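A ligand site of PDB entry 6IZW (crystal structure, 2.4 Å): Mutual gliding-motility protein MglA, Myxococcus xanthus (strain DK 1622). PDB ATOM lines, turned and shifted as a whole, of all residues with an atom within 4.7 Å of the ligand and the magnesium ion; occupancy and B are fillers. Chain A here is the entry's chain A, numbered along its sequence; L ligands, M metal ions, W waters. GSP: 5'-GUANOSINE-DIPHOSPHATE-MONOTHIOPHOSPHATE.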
ATOM      1  N   PRO A  20      15.080  -5.997  -8.741  1.00  0.00           N
ATOM      2  CA  PRO A  20      14.534  -5.031  -7.789  1.00  0.00           C
ATOM      3  C   PRO A  20      15.633  -4.466  -6.889  1.00  0.00           C
ATOM      4  O   PRO A  20      16.792  -4.904  -6.925  1.00  0.00           O
ATOM      5  CB  PRO A  20      13.523  -5.846  -6.977  1.00  0.00           C
ATOM      6  CG  PRO A  20      14.097  -7.241  -7.025  1.00  0.00           C
ATOM      7  CD  PRO A  20      14.714  -7.384  -8.396  1.00  0.00           C
ATOM      8  N   GLY A  21      15.224  -3.506  -6.049  1.00  0.00           N
ATOM      9  CA  GLY A  21      16.174  -2.862  -5.151  1.00  0.00           C
ATOM     10  C   GLY A  21      16.732  -3.863  -4.147  1.00  0.00           C
ATOM     11  O   GLY A  21      16.016  -4.725  -3.621  1.00  0.00           O
ATOM     12  N   LEU A  22      18.049  -3.743  -3.897  1.00  0.00           N
ATOM     13  CA  LEU A  22      18.784  -4.549  -2.918  1.00  0.00           C
ATOM     14  C   LEU A  22      18.854  -6.021  -3.291  1.00  0.00           C
ATOM     15  O   LEU A  22      19.056  -6.868  -2.416  1.00  0.00           O
ATOM     16  CB  LEU A  22      18.196  -4.434  -1.498  1.00  0.00           C
ATOM     17  CG  LEU A  22      17.995  -3.087  -0.800  1.00  0.00           C
ATOM     18  CD1 LEU A  22      17.245  -3.309   0.532  1.00  0.00           C
ATOM     19  CD2 LEU A  22      19.319  -2.344  -0.559  1.00  0.00           C
ATOM     20  N   CYS A  23      18.663  -6.382  -4.551  1.00  0.00           N
ATOM     21  CA  CYS A  23      18.625  -7.819  -4.817  1.00  0.00           C
ATOM     22  C   CYS A  23      19.992  -8.445  -4.997  1.00  0.00           C
ATOM     23  O   CYS A  23      20.089  -9.676  -4.982  1.00  0.00           O
ATOM     24  CB  CYS A  23      17.764  -8.113  -6.054  1.00  0.00           C
ATOM     25  SG  CYS A  23      18.508  -7.521  -7.570  1.00  0.00           S
ATOM     26  N   GLY A  24      21.059  -7.643  -5.179  1.00  0.00           N
ATOM     27  CA  GLY A  24      22.416  -8.162  -5.328  1.00  0.00           C
ATOM     28  C   GLY A  24      23.142  -7.886  -6.632  1.00  0.00           C
ATOM     29  O   GLY A  24      24.211  -8.461  -6.875  1.00  0.00           O
ATOM     30  N   LYS A  25      22.585  -7.028  -7.506  1.00  0.00           N
ATOM     31  CA  LYS A  25      23.215  -6.741  -8.796  1.00  0.00           C
ATOM     32  C   LYS A  25      24.635  -6.209  -8.611  1.00  0.00           C
ATOM     33  O   LYS A  25      25.568  -6.669  -9.264  1.00  0.00           O
ATOM     34  CB  LYS A  25      22.396  -5.712  -9.573  1.00  0.00           C
ATOM     35  CG  LYS A  25      20.957  -6.074  -9.895  1.00  0.00           C
ATOM     36  CD  LYS A  25      20.320  -4.930 -10.692  1.00  0.00           C
ATOM     37  CE  LYS A  25      19.303  -4.124  -9.912  1.00  0.00           C
ATOM     38  NZ  LYS A  25      19.596  -3.795  -8.526  1.00  0.00           N
ATOM     39  N   THR A  26      24.789  -5.212  -7.745  1.00  0.00           N
ATOM     40  CA  THR A  26      26.086  -4.552  -7.598  1.00  0.00           C
ATOM     41  C   THR A  26      27.097  -5.476  -6.939  1.00  0.00           C
ATOM     42  O   THR A  26      28.291  -5.437  -7.266  1.00  0.00           O
ATOM     43  CB  THR A  26      25.906  -3.287  -6.767  1.00  0.00           C
ATOM     44  OG1 THR A  26      25.179  -2.330  -7.541  1.00  0.00           O
ATOM     45  CG2 THR A  26      27.253  -2.715  -6.303  1.00  0.00           C
ATOM     46  N   THR A  27      26.630  -6.324  -6.019  1.00  0.00           N
ATOM     47  CA  THR A  27      27.465  -7.336  -5.393  1.00  0.00           C
ATOM     48  C   THR A  27      28.028  -8.303  -6.442  1.00  0.00           C
ATOM     49  O   THR A  27      29.182  -8.743  -6.325  1.00  0.00           O
ATOM     50  CB  THR A  27      26.643  -8.047  -4.321  1.00  0.00           C
ATOM     51  OG1 THR A  27      26.094  -7.059  -3.437  1.00  0.00           O
ATOM     52  CG2 THR A  27      27.485  -9.048  -3.505  1.00  0.00           C
ATOM     53  N   ASP A  52      24.890   3.274  -0.351  1.00  0.00           N
ATOM     54  CA  ASP A  52      25.403   2.326  -1.338  1.00  0.00           C
ATOM     55  C   ASP A  52      24.370   1.821  -2.329  1.00  0.00           C
ATOM     56  O   ASP A  52      24.668   0.921  -3.142  1.00  0.00           O
ATOM     57  CB  ASP A  52      26.066   1.123  -0.651  1.00  0.00           C
ATOM     58  CG  ASP A  52      27.381   1.484  -0.016  1.00  0.00           C
ATOM     59  OD1 ASP A  52      28.064   2.397  -0.542  1.00  0.00           O
ATOM     60  OD2 ASP A  52      27.731   0.850   1.002  1.00  0.00           O
ATOM     61  N   ARG A  53      23.154   2.344  -2.304  1.00  0.00           N
ATOM     62  CA  ARG A  53      22.206   2.008  -3.350  1.00  0.00           C
ATOM     63  C   ARG A  53      22.664   2.638  -4.657  1.00  0.00           C
ATOM     64  O   ARG A  53      23.132   3.781  -4.686  1.00  0.00           O
ATOM     65  CB  ARG A  53      20.809   2.494  -2.962  1.00  0.00           C
ATOM     66  CG  ARG A  53      20.505   2.030  -1.589  1.00  0.00           C
ATOM     67  CD  ARG A  53      19.109   2.309  -1.193  1.00  0.00           C
ATOM     68  NE  ARG A  53      18.249   1.267  -1.698  1.00  0.00           N
ATOM     69  CZ  ARG A  53      17.174   0.817  -1.065  1.00  0.00           C
ATOM     70  NH1 ARG A  53      16.829   1.316   0.114  1.00  0.00           N
ATOM     71  NH2 ARG A  53      16.466  -0.147  -1.630  1.00  0.00           N
ATOM     72  N   THR A  54      22.589   1.870  -5.731  1.00  0.00           N
ATOM     73  CA  THR A  54      22.953   2.392  -7.020  1.00  0.00           C
ATOM     74  C   THR A  54      21.942   3.456  -7.439  1.00  0.00           C
ATOM     75  O   THR A  54      20.728   3.257  -7.369  1.00  0.00           O
ATOM     76  CB  THR A  54      23.013   1.270  -8.047  1.00  0.00           C
ATOM     77  OG1 THR A  54      23.889   0.252  -7.551  1.00  0.00           O
ATOM     78  CG2 THR A  54      23.496   1.781  -9.396  1.00  0.00           C
ATOM     79  N   ASP A  58      26.208   1.030 -12.131  1.00  0.00           N
ATOM     80  CA  ASP A  58      27.577   0.549 -12.012  1.00  0.00           C
ATOM     81  C   ASP A  58      28.063   0.167 -13.402  1.00  0.00           C
ATOM     82  O   ASP A  58      27.289  -0.305 -14.235  1.00  0.00           O
ATOM     83  CB  ASP A  58      27.744  -0.706 -11.130  1.00  0.00           C
ATOM     84  CG  ASP A  58      27.159  -0.578  -9.737  1.00  0.00           C
ATOM     85  OD1 ASP A  58      27.714   0.195  -8.909  1.00  0.00           O
ATOM     86  OD2 ASP A  58      26.179  -1.295  -9.440  1.00  0.00           O
ATOM     87  N   THR A  78      24.989  -2.507 -14.102  1.00  0.00           N
ATOM     88  CA  THR A  78      23.805  -2.736 -13.292  1.00  0.00           C
ATOM     89  C   THR A  78      22.945  -1.478 -13.311  1.00  0.00           C
ATOM     90  O   THR A  78      23.450  -0.365 -13.453  1.00  0.00           O
ATOM     91  CB  THR A  78      24.167  -3.097 -11.833  1.00  0.00           C
ATOM     92  OG1 THR A  78      24.287  -1.897 -11.052  1.00  0.00           O
ATOM     93  CG2 THR A  78      25.471  -3.878 -11.784  1.00  0.00           C
ATOM     94  N   VAL A  79      21.642  -1.667 -13.162  1.00  0.00           N
ATOM     95  CA  VAL A  79      20.696  -0.551 -13.134  1.00  0.00           C
ATOM     96  C   VAL A  79      20.416  -0.198 -11.681  1.00  0.00           C
ATOM     97  O   VAL A  79      20.698  -1.008 -10.786  1.00  0.00           O
ATOM     98  CB  VAL A  79      19.395  -0.924 -13.876  1.00  0.00           C
ATOM     99  CG1 VAL A  79      19.689  -1.342 -15.300  1.00  0.00           C
ATOM    100  CG2 VAL A  79      18.644  -2.041 -13.108  1.00  0.00           C
ATOM    101  N   PRO A  80      19.860   0.977 -11.397  1.00  0.00           N
ATOM    102  CA  PRO A  80      19.263   1.224 -10.073  1.00  0.00           C
ATOM    103  C   PRO A  80      17.913   0.529  -9.988  1.00  0.00           C
ATOM    104  O   PRO A  80      17.088   0.632 -10.906  1.00  0.00           O
ATOM    105  CB  PRO A  80      19.120   2.739 -10.016  1.00  0.00           C
ATOM    106  CG  PRO A  80      19.030   3.163 -11.451  1.00  0.00           C
ATOM    107  CD  PRO A  80      19.842   2.187 -12.241  1.00  0.00           C
ATOM    108  N   GLY A  81      17.703  -0.208  -8.901  1.00  0.00           N
ATOM    109  CA  GLY A  81      16.600  -1.122  -8.833  1.00  0.00           C
ATOM    110  C   GLY A  81      15.358  -0.599  -8.158  1.00  0.00           C
ATOM    111  O   GLY A  81      14.278  -1.156  -8.361  1.00  0.00           O
ATOM    112  N   GLN A  82      15.483   0.453  -7.350  1.00  0.00           N
ATOM    113  CA  GLN A  82      14.303   0.993  -6.694  1.00  0.00           C
ATOM    114  C   GLN A  82      13.348   1.545  -7.736  1.00  0.00           C
ATOM    115  O   GLN A  82      13.773   2.127  -8.735  1.00  0.00           O
ATOM    116  CB  GLN A  82      14.705   2.072  -5.682  1.00  0.00           C
ATOM    117  CG  GLN A  82      15.418   1.475  -4.474  1.00  0.00           C
ATOM    118  CD  GLN A  82      15.852   2.518  -3.481  1.00  0.00           C
ATOM    119  OE1 GLN A  82      16.950   3.082  -3.591  1.00  0.00           O
ATOM    120  NE2 GLN A  82      14.996   2.790  -2.498  1.00  0.00           N
ATOM    121  N   ASN A 141      19.284 -15.103  -6.488  1.00  0.00           N
ATOM    122  CA  ASN A 141      20.297 -14.704  -5.547  1.00  0.00           C
ATOM    123  C   ASN A 141      19.751 -14.792  -4.109  1.00  0.00           C
ATOM    124  O   ASN A 141      18.554 -14.908  -3.878  1.00  0.00           O
ATOM    125  CB  ASN A 141      20.783 -13.286  -5.870  1.00  0.00           C
ATOM    126  CG  ASN A 141      22.081 -12.934  -5.148  1.00  0.00           C
ATOM    127  OD1 ASN A 141      22.935 -13.798  -4.952  1.00  0.00           O
ATOM    128  ND2 ASN A 141      22.201 -11.672  -4.696  1.00  0.00           N
ATOM    129  N   LYS A 142      20.669 -14.770  -3.132  1.00  0.00           N
ATOM    130  CA  LYS A 142      20.369 -14.823  -1.688  1.00  0.00           C
ATOM    131  C   LYS A 142      19.846 -16.184  -1.261  1.00  0.00           C
ATOM    132  O   LYS A 142      19.003 -16.284  -0.364  1.00  0.00           O
ATOM    133  CB  LYS A 142      19.395 -13.718  -1.245  1.00  0.00           C
ATOM    134  CG  LYS A 142      19.785 -12.322  -1.721  1.00  0.00           C
ATOM    135  CD  LYS A 142      19.157 -11.240  -0.888  1.00  0.00           C
ATOM    136  CE  LYS A 142      19.589  -9.888  -1.387  1.00  0.00           C
ATOM    137  NZ  LYS A 142      19.111  -8.760  -0.533  1.00  0.00           N
ATOM    138  N   ASP A 144      21.343 -18.184   0.540  1.00  0.00           N
ATOM    139  CA  ASP A 144      21.802 -18.493   1.882  1.00  0.00           C
ATOM    140  C   ASP A 144      20.767 -18.152   2.945  1.00  0.00           C
ATOM    141  O   ASP A 144      20.812 -18.731   4.026  1.00  0.00           O
ATOM    142  CB  ASP A 144      23.089 -17.741   2.195  1.00  0.00           C
ATOM    143  CG  ASP A 144      22.975 -16.261   1.899  1.00  0.00           C
ATOM    144  OD1 ASP A 144      22.466 -15.902   0.799  1.00  0.00           O
ATOM    145  OD2 ASP A 144      23.400 -15.452   2.750  1.00  0.00           O
ATOM    146  N   LEU A 145      19.868 -17.216   2.653  1.00  0.00           N
ATOM    147  CA  LEU A 145      19.043 -16.630   3.705  1.00  0.00           C
ATOM    148  C   LEU A 145      17.990 -17.631   4.185  1.00  0.00           C
ATOM    149  O   LEU A 145      17.461 -18.416   3.387  1.00  0.00           O
ATOM    150  CB  LEU A 145      18.356 -15.355   3.218  1.00  0.00           C
ATOM    151  CG  LEU A 145      19.259 -14.131   3.058  1.00  0.00           C
ATOM    152  CD1 LEU A 145      18.493 -12.947   2.474  1.00  0.00           C
ATOM    153  CD2 LEU A 145      19.907 -13.756   4.388  1.00  0.00           C
ATOM    154  N   ALA A 168      22.568 -18.301  -6.719  1.00  0.00           N
ATOM    155  CA  ALA A 168      23.749 -17.560  -6.366  1.00  0.00           C
ATOM    156  C   ALA A 168      23.681 -17.158  -4.906  1.00  0.00           C
ATOM    157  O   ALA A 168      22.615 -17.062  -4.291  1.00  0.00           O
ATOM    158  CB  ALA A 168      23.919 -16.316  -7.248  1.00  0.00           C
ATOM    159  N   VAL A 169      24.870 -16.891  -4.370  1.00  0.00           N
ATOM    160  CA  VAL A 169      25.028 -16.104  -3.149  1.00  0.00           C
ATOM    161  C   VAL A 169      26.121 -15.098  -3.501  1.00  0.00           C
ATOM    162  O   VAL A 169      27.308 -15.376  -3.347  1.00  0.00           O
ATOM    163  CB  VAL A 169      25.428 -16.976  -1.953  1.00  0.00           C
ATOM    164  CG1 VAL A 169      25.684 -16.101  -0.718  1.00  0.00           C
ATOM    165  CG2 VAL A 169      24.356 -18.099  -1.730  1.00  0.00           C
ATOM    166  N   ALA A 170      25.714 -13.948  -4.041  1.00  0.00           N
ATOM    167  CA  ALA A 170      26.666 -13.032  -4.657  1.00  0.00           C
ATOM    168  C   ALA A 170      27.831 -12.661  -3.740  1.00  0.00           C
ATOM    169  O   ALA A 170      28.972 -12.715  -4.232  1.00  0.00           O
ATOM    170  CB  ALA A 170      25.926 -11.786  -5.187  1.00  0.00           C
ATOM    171  N   PRO A 171      27.658 -12.337  -2.444  1.00  0.00           N
ATOM    172  CA  PRO A 171      28.820 -11.929  -1.613  1.00  0.00           C
ATOM    173  C   PRO A 171      29.892 -13.013  -1.438  1.00  0.00           C
ATOM    174  O   PRO A 171      31.045 -12.676  -1.160  1.00  0.00           O
ATOM    175  CB  PRO A 171      28.191 -11.572  -0.247  1.00  0.00           C
ATOM    176  CG  PRO A 171      26.704 -11.346  -0.550  1.00  0.00           C
ATOM    177  CD  PRO A 171      26.410 -12.361  -1.642  1.00  0.00           C
HETATM  178  PG  GSP L   1      20.221  -1.401  -5.739  1.00  0.00           P
HETATM  179  O3B GSP L   1      20.663  -2.810  -5.083  1.00  0.00           O
HETATM  180  S1G GSP L   1      19.397  -0.494  -4.482  1.00  0.00           S
HETATM  181  O2G GSP L   1      19.244  -1.709  -6.834  1.00  0.00           O
HETATM  182  O3G GSP L   1      21.424  -0.638  -6.309  1.00  0.00           O
HETATM  183  PB  GSP L   1      21.566  -4.010  -5.654  1.00  0.00           P
HETATM  184  O1B GSP L   1      22.761  -3.555  -6.389  1.00  0.00           O
HETATM  185  O2B GSP L   1      20.856  -5.068  -6.392  1.00  0.00           O
HETATM  186  PA  GSP L   1      23.380  -4.763  -3.632  1.00  0.00           P
HETATM  187  O1A GSP L   1      24.227  -5.436  -4.632  1.00  0.00           O
HETATM  188  O2A GSP L   1      23.863  -3.405  -3.284  1.00  0.00           O
HETATM  189  O3A GSP L   1      21.890  -4.682  -4.233  1.00  0.00           O
HETATM  190  O5' GSP L   1      23.123  -5.666  -2.326  1.00  0.00           O
HETATM  191  C5' GSP L   1      22.177  -5.231  -1.364  1.00  0.00           C
HETATM  192  C4' GSP L   1      22.452  -5.820   0.015  1.00  0.00           C
HETATM  193  O4' GSP L   1      22.171  -7.207  -0.022  1.00  0.00           O
HETATM  194  C3' GSP L   1      23.926  -5.698   0.399  1.00  0.00           C
HETATM  195  O3' GSP L   1      23.984  -5.543   1.806  1.00  0.00           O
HETATM  196  C2' GSP L   1      24.505  -7.048   0.018  1.00  0.00           C
HETATM  197  O2' GSP L   1      25.639  -7.416   0.778  1.00  0.00           O
HETATM  198  C1' GSP L   1      23.327  -7.954   0.314  1.00  0.00           C
HETATM  199  N9  GSP L   1      23.373  -9.180  -0.485  1.00  0.00           N
HETATM  200  C8  GSP L   1      23.574  -9.250  -1.848  1.00  0.00           C
HETATM  201  N7  GSP L   1      23.529 -10.559  -2.196  1.00  0.00           N
HETATM  202  C5  GSP L   1      23.304 -11.311  -1.088  1.00  0.00           C
HETATM  203  C6  GSP L   1      23.189 -12.676  -0.886  1.00  0.00           C
HETATM  204  O6  GSP L   1      23.287 -13.440  -1.843  1.00  0.00           O
HETATM  205  N1  GSP L   1      22.972 -13.195   0.363  1.00  0.00           N
HETATM  206  C2  GSP L   1      22.857 -12.327   1.431  1.00  0.00           C
HETATM  207  N2  GSP L   1      22.647 -12.835   2.646  1.00  0.00           N
HETATM  208  N3  GSP L   1      22.997 -10.958   1.241  1.00  0.00           N
HETATM  209  C4  GSP L   1      23.208 -10.460  -0.005  1.00  0.00           C
HETATM  210 MG    MG M   1      23.300  -1.501  -6.819  1.00  0.00          MG
HETATM  211  O   HOH W   1      22.765  -2.690   1.735  1.00  0.00           O
HETATM  212  O   HOH W   2      22.524  -7.033   3.361  1.00  0.00           O
HETATM  213  O   HOH W   3      21.836  -1.369  -2.467  1.00  0.00           O
HETATM  214  O   HOH W   4      25.978  -2.822  -1.827  1.00  0.00           O
HETATM  215  O   HOH W   5      22.758  -1.694  -8.815  1.00  0.00           O
HETATM  216  O   HOH W   6      24.140  -1.199  -4.931  1.00  0.00           O
HETATM  217  O   HOH W   7      18.479   1.599  -6.516  1.00  0.00           O
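The backbone NH (N) of Thr 54 lies close to an oxygen (O3G) of the ligand (2.8 Å). An oxygen (O1A) of the ligand lies within hydrogen-bond range of the backbone NH (N) of Thr 26 (3.2 Å). An oxygen (O2B) of the ligand is in hydrogen-bond range of the backbone NH (N) of Lys 25, 2.8 Å away. The side-chain amino group of Lys 25 lies within salt-bridge range of an oxygen (O2B) of the ligand, 2.8 Å away. OD2 of Asp 144 sits at hydrogen-bond distance from N2 of the ligand (2.7 Å). An oxygen (O1A) of the ligand is in hydrogen-bond range of the backbone NH of Thr 27, 2.9 Å away. O1A of the ligand sits at hydrogen-bond distance from OG1 of Thr 27. N of Gly 24 sits at hydrogen-bond distance from O2B of the ligand (2.9 Å). O2G of the ligand sits at hydrogen-bond distance from N of Gly 81 (3.0 Å). N of Leu 22 is in hydrogen-bond range of O3B of the ligand (3.0 Å). A nitrogen (N7) of the ligand lies within hydrogen-bond range of the side-chain amide nitrogen of Asn 141, 3.0 Å away. The backbone NH of Cys 23 sits at hydrogen-bond distance from an oxygen (O2B) of the ligand (3.2 Å). The side-chain sulfur of Cys 23 is in hydrogen-bond range of an oxygen (O2B) of the ligand, at 3.6 Å. N of Lys 142 is in hydrogen-bond range of O6 of the ligand, 3.2 Å away. The side-chain amino group of Lys 142 is in hydrogen-bond range of an oxygen (O4') of the ligand. The backbone NH (N) of Ala 170 is in hydrogen-bond range of an oxygen (O6) of the ligand (3.3 Å). NE of Arg 53 sits close to S1G of the ligand, 3.5 Å away.
The side-chain hydroxyl of Thr 54 sits close to the side-chain carboxylate of Asp 58 (3.3 Å). O of Pro 20 is in hydrogen-bond range of NZ of Lys 25 (3.4 Å). The backbone NH of Gly 21 is in hydrogen-bond range of the backbone carbonyl oxygen of Gly 81 (3.4 Å). The backbone carbonyl oxygen (O) of Leu 22 sits at hydrogen-bond distance from the side-chain amino group (NZ) of Lys 142 (2.7 Å). The backbone carbonyl oxygen (O) of Ala 168 lies close to the side-chain amide oxygen (OD1) of Asn 141 (3.3 Å). The side-chain sulfur (SG) of Cys 23 lies within hydrogen-bond range of the backbone carbonyl oxygen (O) of Pro 20 (3.2 Å). The guanidinium group of Arg 53 sits at hydrogen-bond distance from the side-chain amide oxygen of Gln 82. The side-chain carboxylate (OD2) of Asp 58 is in hydrogen-bond range of the side-chain hydroxyl (OG1) of Thr 78, 2.6 Å away.
Residues that only touch the ligand: Pro 171, Leu 145, Val 169 and Gly 21. 17 residues have an atom within 4 Å of the ligand: Gly 21, Leu 22, Cys 23, Gly 24, Lys 25, Thr 26, Thr 27, Arg 53, Thr 54, Gly 81, Asn 141, Lys 142, Asp 144, Leu 145, Val 169, Ala 170 and Pro 171.
Residues that only touch the magnesium ion: Asp 58 (3.9 Å).
The magnesium ion is bound by the side-chain hydroxyl (OG1) of Thr 54 (2.0 Å), water W5 (2.1 Å), water W6 (2.1 Å), an oxygen (O3G) of the ligand (2.1 Å), an oxygen (O1B) of the ligand (2.2 Å) and the side-chain hydroxyl (OG1) of Thr 26 (2.2 Å).
Water W5 lies within hydrogen-bond range of the side-chain hydroxyl (OG1) of Thr 78 (2.7 Å), the backbone carbonyl oxygen (O) of Val 79 (2.9 Å) and the side-chain carboxylate (OD2) of Asp 58 (3.5 Å). Water W6 lies within hydrogen-bond range of O2A of the ligand (2.8 Å) and O of Asp 52 (2.8 Å). Water W7 lies within hydrogen-bond range of the backbone carbonyl oxygen of Thr 54 (2.9 Å), a sulfur (S1G) of the ligand (3.1 Å), the backbone NH of Gly 81 (3.1 Å) and the backbone NH of Gln 82 (3.3 Å).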
